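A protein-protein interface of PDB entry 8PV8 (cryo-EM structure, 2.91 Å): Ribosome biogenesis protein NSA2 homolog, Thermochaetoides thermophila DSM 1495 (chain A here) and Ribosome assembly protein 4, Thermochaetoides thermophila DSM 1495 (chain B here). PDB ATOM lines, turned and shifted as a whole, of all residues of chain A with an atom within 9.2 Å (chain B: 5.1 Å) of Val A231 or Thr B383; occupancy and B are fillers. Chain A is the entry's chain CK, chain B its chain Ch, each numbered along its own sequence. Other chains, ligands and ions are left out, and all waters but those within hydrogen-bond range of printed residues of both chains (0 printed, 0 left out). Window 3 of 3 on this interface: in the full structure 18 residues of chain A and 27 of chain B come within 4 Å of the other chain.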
ATOM      1  N   VAL A 225      31.173 -22.786  20.147  1.00  0.00           N
ATOM      2  CA  VAL A 225      30.220 -23.093  19.088  1.00  0.00           C
ATOM      3  C   VAL A 225      29.175 -21.990  18.984  1.00  0.00           C
ATOM      4  O   VAL A 225      28.026 -22.243  18.605  1.00  0.00           O
ATOM      5  CB  VAL A 225      29.561 -24.462  19.321  1.00  0.00           C
ATOM      6  CG1 VAL A 225      30.548 -25.573  19.021  1.00  0.00           C
ATOM      7  CG2 VAL A 225      29.067 -24.574  20.751  1.00  0.00           C
ATOM      8  N   SER A 226      29.565 -20.760  19.328  1.00  0.00           N
ATOM      9  CA  SER A 226      28.649 -19.627  19.244  1.00  0.00           C
ATOM     10  C   SER A 226      28.257 -19.293  17.810  1.00  0.00           C
ATOM     11  O   SER A 226      27.179 -18.731  17.590  1.00  0.00           O
ATOM     12  CB  SER A 226      29.274 -18.397  19.901  1.00  0.00           C
ATOM     13  OG  SER A 226      29.559 -18.635  21.266  1.00  0.00           O
ATOM     14  N   LEU A 228      27.609 -21.410  15.400  1.00  0.00           N
ATOM     15  CA  LEU A 228      26.747 -22.430  14.819  1.00  0.00           C
ATOM     16  C   LEU A 228      25.292 -22.277  15.241  1.00  0.00           C
ATOM     17  O   LEU A 228      24.431 -23.004  14.735  1.00  0.00           O
ATOM     18  CB  LEU A 228      27.257 -23.823  15.187  1.00  0.00           C
ATOM     19  CG  LEU A 228      28.595 -24.212  14.562  1.00  0.00           C
ATOM     20  CD1 LEU A 228      29.394 -25.066  15.522  1.00  0.00           C
ATOM     21  CD2 LEU A 228      28.377 -24.942  13.247  1.00  0.00           C
ATOM     22  N   GLY A 229      25.000 -21.345  16.143  1.00  0.00           N
ATOM     23  CA  GLY A 229      23.633 -21.115  16.583  1.00  0.00           C
ATOM     24  C   GLY A 229      23.019 -22.266  17.350  1.00  0.00           C
ATOM     25  O   GLY A 229      21.812 -22.514  17.233  1.00  0.00           O
ATOM     26  N   ILE A 230      23.820 -22.975  18.134  1.00  0.00           N
ATOM     27  CA  ILE A 230      23.326 -24.070  18.958  1.00  0.00           C
ATOM     28  C   ILE A 230      22.675 -23.486  20.201  1.00  0.00           C
ATOM     29  O   ILE A 230      23.271 -22.663  20.906  1.00  0.00           O
ATOM     30  CB  ILE A 230      24.462 -25.043  19.323  1.00  0.00           C
ATOM     31  CG1 ILE A 230      25.223 -25.466  18.066  1.00  0.00           C
ATOM     32  CG2 ILE A 230      23.907 -26.263  20.039  1.00  0.00           C
ATOM     33  CD1 ILE A 230      26.360 -26.423  18.334  1.00  0.00           C
ATOM     34  N   VAL A 231      21.440 -23.908  20.470  1.00  0.00           N
ATOM     35  CA  VAL A 231      20.644 -23.353  21.555  1.00  0.00           C
ATOM     36  C   VAL A 231      19.994 -24.509  22.309  1.00  0.00           C
ATOM     37  O   VAL A 231      19.784 -25.597  21.768  1.00  0.00           O
ATOM     38  CB  VAL A 231      19.591 -22.349  21.013  1.00  0.00           C
ATOM     39  CG1 VAL A 231      18.485 -23.064  20.250  1.00  0.00           C
ATOM     40  CG2 VAL A 231      19.040 -21.449  22.108  1.00  0.00           C
ATOM     41  N   THR A 232      19.711 -24.276  23.589  1.00  0.00           N
ATOM     42  CA  THR A 232      19.051 -25.274  24.414  1.00  0.00           C
ATOM     43  C   THR A 232      17.533 -25.150  24.278  1.00  0.00           C
ATOM     44  O   THR A 232      17.014 -24.410  23.440  1.00  0.00           O
ATOM     45  CB  THR A 232      19.496 -25.143  25.869  1.00  0.00           C
ATOM     46  OG1 THR A 232      18.998 -26.253  26.624  1.00  0.00           O
ATOM     47  CG2 THR A 232      18.982 -23.854  26.474  1.00  0.00           C
ATOM     48  N   ALA A 233      16.810 -25.886  25.122  1.00  0.00           N
ATOM     49  CA  ALA A 233      15.359 -25.982  25.039  1.00  0.00           C
ATOM     50  C   ALA A 233      14.627 -24.721  25.484  1.00  0.00           C
ATOM     51  O   ALA A 233      13.409 -24.650  25.308  1.00  0.00           O
ATOM     52  CB  ALA A 233      14.870 -27.171  25.868  1.00  0.00           C
ATOM     53  N   SER A 234      15.311 -23.730  26.059  1.00  0.00           N
ATOM     54  CA  SER A 234      14.635 -22.524  26.517  1.00  0.00           C
ATOM     55  C   SER A 234      15.155 -21.235  25.900  1.00  0.00           C
ATOM     56  O   SER A 234      14.423 -20.240  25.903  1.00  0.00           O
ATOM     57  CB  SER A 234      14.727 -22.396  28.044  1.00  0.00           C
ATOM     58  OG  SER A 234      16.068 -22.231  28.463  1.00  0.00           O
ATOM     59  N   GLY A 235      16.380 -21.211  25.386  1.00  0.00           N
ATOM     60  CA  GLY A 235      16.939 -20.030  24.758  1.00  0.00           C
ATOM     61  C   GLY A 235      18.360 -19.703  25.164  1.00  0.00           C
ATOM     62  O   GLY A 235      18.936 -18.746  24.628  1.00  0.00           O
ATOM     63  N   LYS A 236      18.945 -20.447  26.101  1.00  0.00           N
ATOM     64  CA  LYS A 236      20.327 -20.191  26.487  1.00  0.00           C
ATOM     65  C   LYS A 236      21.273 -20.589  25.362  1.00  0.00           C
ATOM     66  O   LYS A 236      21.125 -21.647  24.746  1.00  0.00           O
ATOM     67  CB  LYS A 236      20.685 -20.955  27.762  1.00  0.00           C
ATOM     68  CG  LYS A 236      19.820 -20.638  28.964  1.00  0.00           C
ATOM     69  CD  LYS A 236      20.253 -21.469  30.160  1.00  0.00           C
ATOM     70  CE  LYS A 236      19.407 -21.171  31.381  1.00  0.00           C
ATOM     71  NZ  LYS A 236      19.766 -22.058  32.521  1.00  0.00           N
ATOM     72  N   ILE A 237      22.255 -19.734  25.101  1.00  0.00           N
ATOM     73  CA  ILE A 237      23.216 -19.981  24.032  1.00  0.00           C
ATOM     74  C   ILE A 237      24.257 -20.978  24.517  1.00  0.00           C
ATOM     75  O   ILE A 237      24.941 -20.742  25.521  1.00  0.00           O
ATOM     76  CB  ILE A 237      23.877 -18.670  23.580  1.00  0.00           C
ATOM     77  CG1 ILE A 237      22.837 -17.720  22.993  1.00  0.00           C
ATOM     78  CG2 ILE A 237      24.974 -18.950  22.567  1.00  0.00           C
ATOM     79  CD1 ILE A 237      23.361 -16.326  22.766  1.00  0.00           C
ATOM     80  N   ALA A 238      24.381 -22.093  23.806  1.00  0.00           N
ATOM     81  CA  ALA A 238      25.418 -23.078  24.079  1.00  0.00           C
ATOM     82  C   ALA A 238      26.690 -22.655  23.355  1.00  0.00           C
ATOM     83  O   ALA A 238      26.739 -22.673  22.121  1.00  0.00           O
ATOM     84  CB  ALA A 238      24.977 -24.470  23.634  1.00  0.00           C
ATOM     85  N   TRP A 239      27.708 -22.264  24.118  1.00  0.00           N
ATOM     86  CA  TRP A 239      28.950 -21.763  23.548  1.00  0.00           C
ATOM     87  C   TRP A 239      30.149 -22.650  23.842  1.00  0.00           C
ATOM     88  O   TRP A 239      31.285 -22.223  23.621  1.00  0.00           O
ATOM     89  CB  TRP A 239      29.223 -20.339  24.045  1.00  0.00           C
ATOM     90  CG  TRP A 239      29.568 -20.246  25.492  1.00  0.00           C
ATOM     91  CD1 TRP A 239      28.715 -20.373  26.548  1.00  0.00           C
ATOM     92  CD2 TRP A 239      30.860 -19.988  26.049  1.00  0.00           C
ATOM     93  NE1 TRP A 239      29.396 -20.218  27.728  1.00  0.00           N
ATOM     94  CE2 TRP A 239      30.716 -19.979  27.450  1.00  0.00           C
ATOM     95  CE3 TRP A 239      32.127 -19.766  25.501  1.00  0.00           C
ATOM     96  CZ2 TRP A 239      31.788 -19.755  28.307  1.00  0.00           C
ATOM     97  CZ3 TRP A 239      33.188 -19.548  26.353  1.00  0.00           C
ATOM     98  CH2 TRP A 239      33.015 -19.545  27.739  1.00  0.00           C
ATOM     99  N   ARG A 241      31.356 -26.845  23.277  1.00  0.00           N
ATOM    100  CA  ARG A 241      30.968 -28.182  22.851  1.00  0.00           C
ATOM    101  C   ARG A 241      32.218 -28.980  22.504  1.00  0.00           C
ATOM    102  O   ARG A 241      33.218 -28.432  22.039  1.00  0.00           O
ATOM    103  CB  ARG A 241      29.986 -28.111  21.670  1.00  0.00           C
ATOM    104  CG  ARG A 241      29.459 -29.446  21.172  1.00  0.00           C
ATOM    105  CD  ARG A 241      28.203 -29.273  20.341  1.00  0.00           C
ATOM    106  NE  ARG A 241      27.000 -29.371  21.158  1.00  0.00           N
ATOM    107  CZ  ARG A 241      26.394 -30.511  21.461  1.00  0.00           C
ATOM    108  NH1 ARG A 241      26.860 -31.675  21.038  1.00  0.00           N
ATOM    109  NH2 ARG A 241      25.295 -30.482  22.208  1.00  0.00           N
ATOM    110  N   HIS B 320      17.803 -19.166  11.509  1.00  0.00           N
ATOM    111  CA  HIS B 320      17.787 -20.526  12.025  1.00  0.00           C
ATOM    112  C   HIS B 320      19.204 -21.074  12.142  1.00  0.00           C
ATOM    113  O   HIS B 320      20.116 -20.642  11.431  1.00  0.00           O
ATOM    114  CB  HIS B 320      16.951 -21.430  11.124  1.00  0.00           C
ATOM    115  CG  HIS B 320      15.476 -21.211  11.250  1.00  0.00           C
ATOM    116  ND1 HIS B 320      14.773 -21.517  12.395  1.00  0.00           N
ATOM    117  CD2 HIS B 320      14.568 -20.728  10.370  1.00  0.00           C
ATOM    118  CE1 HIS B 320      13.496 -21.231  12.215  1.00  0.00           C
ATOM    119  NE2 HIS B 320      13.346 -20.747  10.996  1.00  0.00           N
ATOM    120  N   SER B 377       8.175 -20.732  10.665  1.00  0.00           N
ATOM    121  CA  SER B 377       9.179 -21.658  10.166  1.00  0.00           C
ATOM    122  C   SER B 377       9.735 -22.472  11.321  1.00  0.00           C
ATOM    123  O   SER B 377      10.210 -21.910  12.312  1.00  0.00           O
ATOM    124  CB  SER B 377      10.315 -20.919   9.454  1.00  0.00           C
ATOM    125  OG  SER B 377      10.816 -19.864  10.255  1.00  0.00           O
ATOM    126  N   ALA B 378       9.680 -23.794  11.189  1.00  0.00           N
ATOM    127  CA  ALA B 378      10.161 -24.712  12.207  1.00  0.00           C
ATOM    128  C   ALA B 378      11.511 -25.269  11.786  1.00  0.00           C
ATOM    129  O   ALA B 378      11.725 -25.551  10.604  1.00  0.00           O
ATOM    130  CB  ALA B 378       9.169 -25.854  12.413  1.00  0.00           C
ATOM    131  N   SER B 379      12.428 -25.434  12.741  1.00  0.00           N
ATOM    132  CA  SER B 379      13.744 -25.929  12.373  1.00  0.00           C
ATOM    133  C   SER B 379      14.207 -27.011  13.337  1.00  0.00           C
ATOM    134  O   SER B 379      13.592 -27.263  14.374  1.00  0.00           O
ATOM    135  CB  SER B 379      14.776 -24.801  12.318  1.00  0.00           C
ATOM    136  OG  SER B 379      14.648 -23.943  13.436  1.00  0.00           O
ATOM    137  N   ASP B 381      16.971 -26.855  14.979  1.00  0.00           N
ATOM    138  CA  ASP B 381      17.671 -26.262  16.109  1.00  0.00           C
ATOM    139  C   ASP B 381      16.774 -26.091  17.328  1.00  0.00           C
ATOM    140  O   ASP B 381      17.022 -25.193  18.140  1.00  0.00           O
ATOM    141  CB  ASP B 381      18.300 -24.920  15.703  1.00  0.00           C
ATOM    142  CG  ASP B 381      17.286 -23.906  15.178  1.00  0.00           C
ATOM    143  OD1 ASP B 381      16.062 -24.143  15.239  1.00  0.00           O
ATOM    144  OD2 ASP B 381      17.723 -22.841  14.700  1.00  0.00           O
ATOM    145  N   PHE B 382      15.712 -26.902  17.424  1.00  0.00           N
ATOM    146  CA  PHE B 382      14.742 -26.991  18.520  1.00  0.00           C
ATOM    147  C   PHE B 382      13.788 -25.805  18.542  1.00  0.00           C
ATOM    148  O   PHE B 382      12.996 -25.676  19.479  1.00  0.00           O
ATOM    149  CB  PHE B 382      15.380 -27.118  19.918  1.00  0.00           C
ATOM    150  CG  PHE B 382      16.315 -28.302  20.103  1.00  0.00           C
ATOM    151  CD1 PHE B 382      16.423 -29.317  19.164  1.00  0.00           C
ATOM    152  CD2 PHE B 382      17.082 -28.389  21.254  1.00  0.00           C
ATOM    153  CE1 PHE B 382      17.282 -30.381  19.361  1.00  0.00           C
ATOM    154  CE2 PHE B 382      17.939 -29.452  21.457  1.00  0.00           C
ATOM    155  CZ  PHE B 382      18.038 -30.448  20.510  1.00  0.00           C
ATOM    156  N   THR B 383      13.828 -24.928  17.537  1.00  0.00           N
ATOM    157  CA  THR B 383      13.149 -23.643  17.626  1.00  0.00           C
ATOM    158  C   THR B 383      12.203 -23.442  16.452  1.00  0.00           C
ATOM    159  O   THR B 383      12.187 -24.208  15.476  1.00  0.00           O
ATOM    160  CB  THR B 383      14.138 -22.471  17.656  1.00  0.00           C
ATOM    161  OG1 THR B 383      14.884 -22.445  16.434  1.00  0.00           O
ATOM    162  CG2 THR B 383      15.101 -22.608  18.812  1.00  0.00           C
ATOM    163  N   MET B 384      11.407 -22.380  16.572  1.00  0.00           N
ATOM    164  CA  MET B 384      10.575 -21.884  15.488  1.00  0.00           C
ATOM    165  C   MET B 384      10.710 -20.371  15.434  1.00  0.00           C
ATOM    166  O   MET B 384      11.087 -19.735  16.417  1.00  0.00           O
ATOM    167  CB  MET B 384       9.113 -22.282  15.686  1.00  0.00           C
ATOM    168  CG  MET B 384       8.867 -23.771  15.589  1.00  0.00           C
ATOM    169  SD  MET B 384       7.131 -24.164  15.773  1.00  0.00           S
ATOM    170  CE  MET B 384       6.975 -23.894  17.535  1.00  0.00           C
ATOM    171  N   TYR B 385      10.407 -19.798  14.277  1.00  0.00           N
ATOM    172  CA  TYR B 385      10.395 -18.353  14.106  1.00  0.00           C
ATOM    173  C   TYR B 385       9.076 -17.916  13.490  1.00  0.00           C
ATOM    174  O   TYR B 385       8.501 -18.631  12.662  1.00  0.00           O
ATOM    175  CB  TYR B 385      11.549 -17.876  13.225  1.00  0.00           C
ATOM    176  CG  TYR B 385      12.822 -17.538  13.965  1.00  0.00           C
ATOM    177  CD1 TYR B 385      12.981 -16.303  14.575  1.00  0.00           C
ATOM    178  CD2 TYR B 385      13.877 -18.435  14.024  1.00  0.00           C
ATOM    179  CE1 TYR B 385      14.145 -15.978  15.242  1.00  0.00           C
ATOM    180  CE2 TYR B 385      15.046 -18.121  14.688  1.00  0.00           C
ATOM    181  CZ  TYR B 385      15.174 -16.891  15.294  1.00  0.00           C
ATOM    182  OH  TYR B 385      16.337 -16.573  15.958  1.00  0.00           O
ATOM    183  N   ARG B 399      10.532 -15.512  18.431  1.00  0.00           N
ATOM    184  CA  ARG B 399      11.124 -16.839  18.358  1.00  0.00           C
ATOM    185  C   ARG B 399      10.374 -17.749  19.319  1.00  0.00           C
ATOM    186  O   ARG B 399      10.297 -17.466  20.520  1.00  0.00           O
ATOM    187  CB  ARG B 399      12.615 -16.816  18.687  1.00  0.00           C
ATOM    188  CG  ARG B 399      13.314 -18.113  18.323  1.00  0.00           C
ATOM    189  CD  ARG B 399      14.810 -18.053  18.552  1.00  0.00           C
ATOM    190  NE  ARG B 399      15.493 -19.108  17.814  1.00  0.00           N
ATOM    191  CZ  ARG B 399      16.797 -19.340  17.865  1.00  0.00           C
ATOM    192  NH1 ARG B 399      17.600 -18.607  18.618  1.00  0.00           N
ATOM    193  NH2 ARG B 399      17.309 -20.333  17.143  1.00  0.00           N
ATOM    194  N   LEU B 400       9.821 -18.828  18.784  1.00  0.00           N
ATOM    195  CA  LEU B 400       9.022 -19.777  19.546  1.00  0.00           C
ATOM    196  C   LEU B 400       9.968 -20.833  20.106  1.00  0.00           C
ATOM    197  O   LEU B 400      10.564 -21.616  19.350  1.00  0.00           O
ATOM    198  CB  LEU B 400       7.934 -20.386  18.662  1.00  0.00           C
ATOM    199  CG  LEU B 400       6.641 -19.594  18.389  1.00  0.00           C
ATOM    200  CD1 LEU B 400       6.849 -18.333  17.561  1.00  0.00           C
ATOM    201  CD2 LEU B 400       5.631 -20.475  17.688  1.00  0.00           C
ATOM    202  N   LEU B 401      10.113 -20.832  21.432  1.00  0.00           N
ATOM    203  CA  LEU B 401      11.092 -21.621  22.165  1.00  0.00           C
ATOM    204  C   LEU B 401      10.380 -22.545  23.140  1.00  0.00           C
ATOM    205  O   LEU B 401       9.365 -22.167  23.733  1.00  0.00           O
ATOM    206  CB  LEU B 401      12.046 -20.713  22.948  1.00  0.00           C
ATOM    207  CG  LEU B 401      12.822 -19.642  22.186  1.00  0.00           C
ATOM    208  CD1 LEU B 401      13.485 -18.677  23.146  1.00  0.00           C
ATOM    209  CD2 LEU B 401      13.864 -20.299  21.331  1.00  0.00           C
ATOM    210  N   VAL B 407      11.689 -29.865  15.674  1.00  0.00           N
ATOM    211  CA  VAL B 407      10.279 -29.591  15.438  1.00  0.00           C
ATOM    212  C   VAL B 407       9.970 -30.012  14.009  1.00  0.00           C
ATOM    213  O   VAL B 407      10.553 -29.479  13.057  1.00  0.00           O
ATOM    214  CB  VAL B 407       9.942 -28.112  15.669  1.00  0.00           C
ATOM    215  CG1 VAL B 407       8.482 -27.853  15.341  1.00  0.00           C
ATOM    216  CG2 VAL B 407      10.270 -27.708  17.089  1.00  0.00           C
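Of chain B, only Asp B381 (3.3 Å), Phe B382 (3.9 Å) and Thr B383 (3.7 Å) come within 4 Å of Val A231. Asp B381 touches just one residue of chain A: Val A231 (3.3 Å). Of the printed residues of chain A, Phe B382 touches Val A231. Of the printed residues of chain A, Leu B401 touches Ser A234. Printed residues of chain B within 4 Å of Ser A234: Leu B401 (3.3 Å). His B320 touches none of the printed residues of chain A. Tyr B385 touches none of the printed residues of chain A.
Asp B381 touches Val A231. O of Val A231 touches CD2 of Phe B382, 3.9 Å away. Val A231 touches Thr B383. Ser A234 touches Leu B401 (O to CD1, 3.3 Å).
Hydrophobic or aromatic side chains of chain B within 4 Å of the printed part of chain A: Phe B382 and Leu B401. Among the printed residues, no Asp or Glu carboxylate lies within 4 Å of a Lys or Arg side-chain nitrogen of the other chain.
The side-chain hydroxyl of Ser B379 is in hydrogen-bond range of the backbone carbonyl oxygen of Thr B383 (3.2 Å). OD2 of Asp B381 is in salt-bridge range of NH2 of Arg B399. The side-chain carboxylate of Asp B381 sits close to the backbone NH of Thr B383, at 3.3 Å. OG1 of Thr B383 lies within hydrogen-bond range of NH2 of Arg B399 (3.3 Å).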
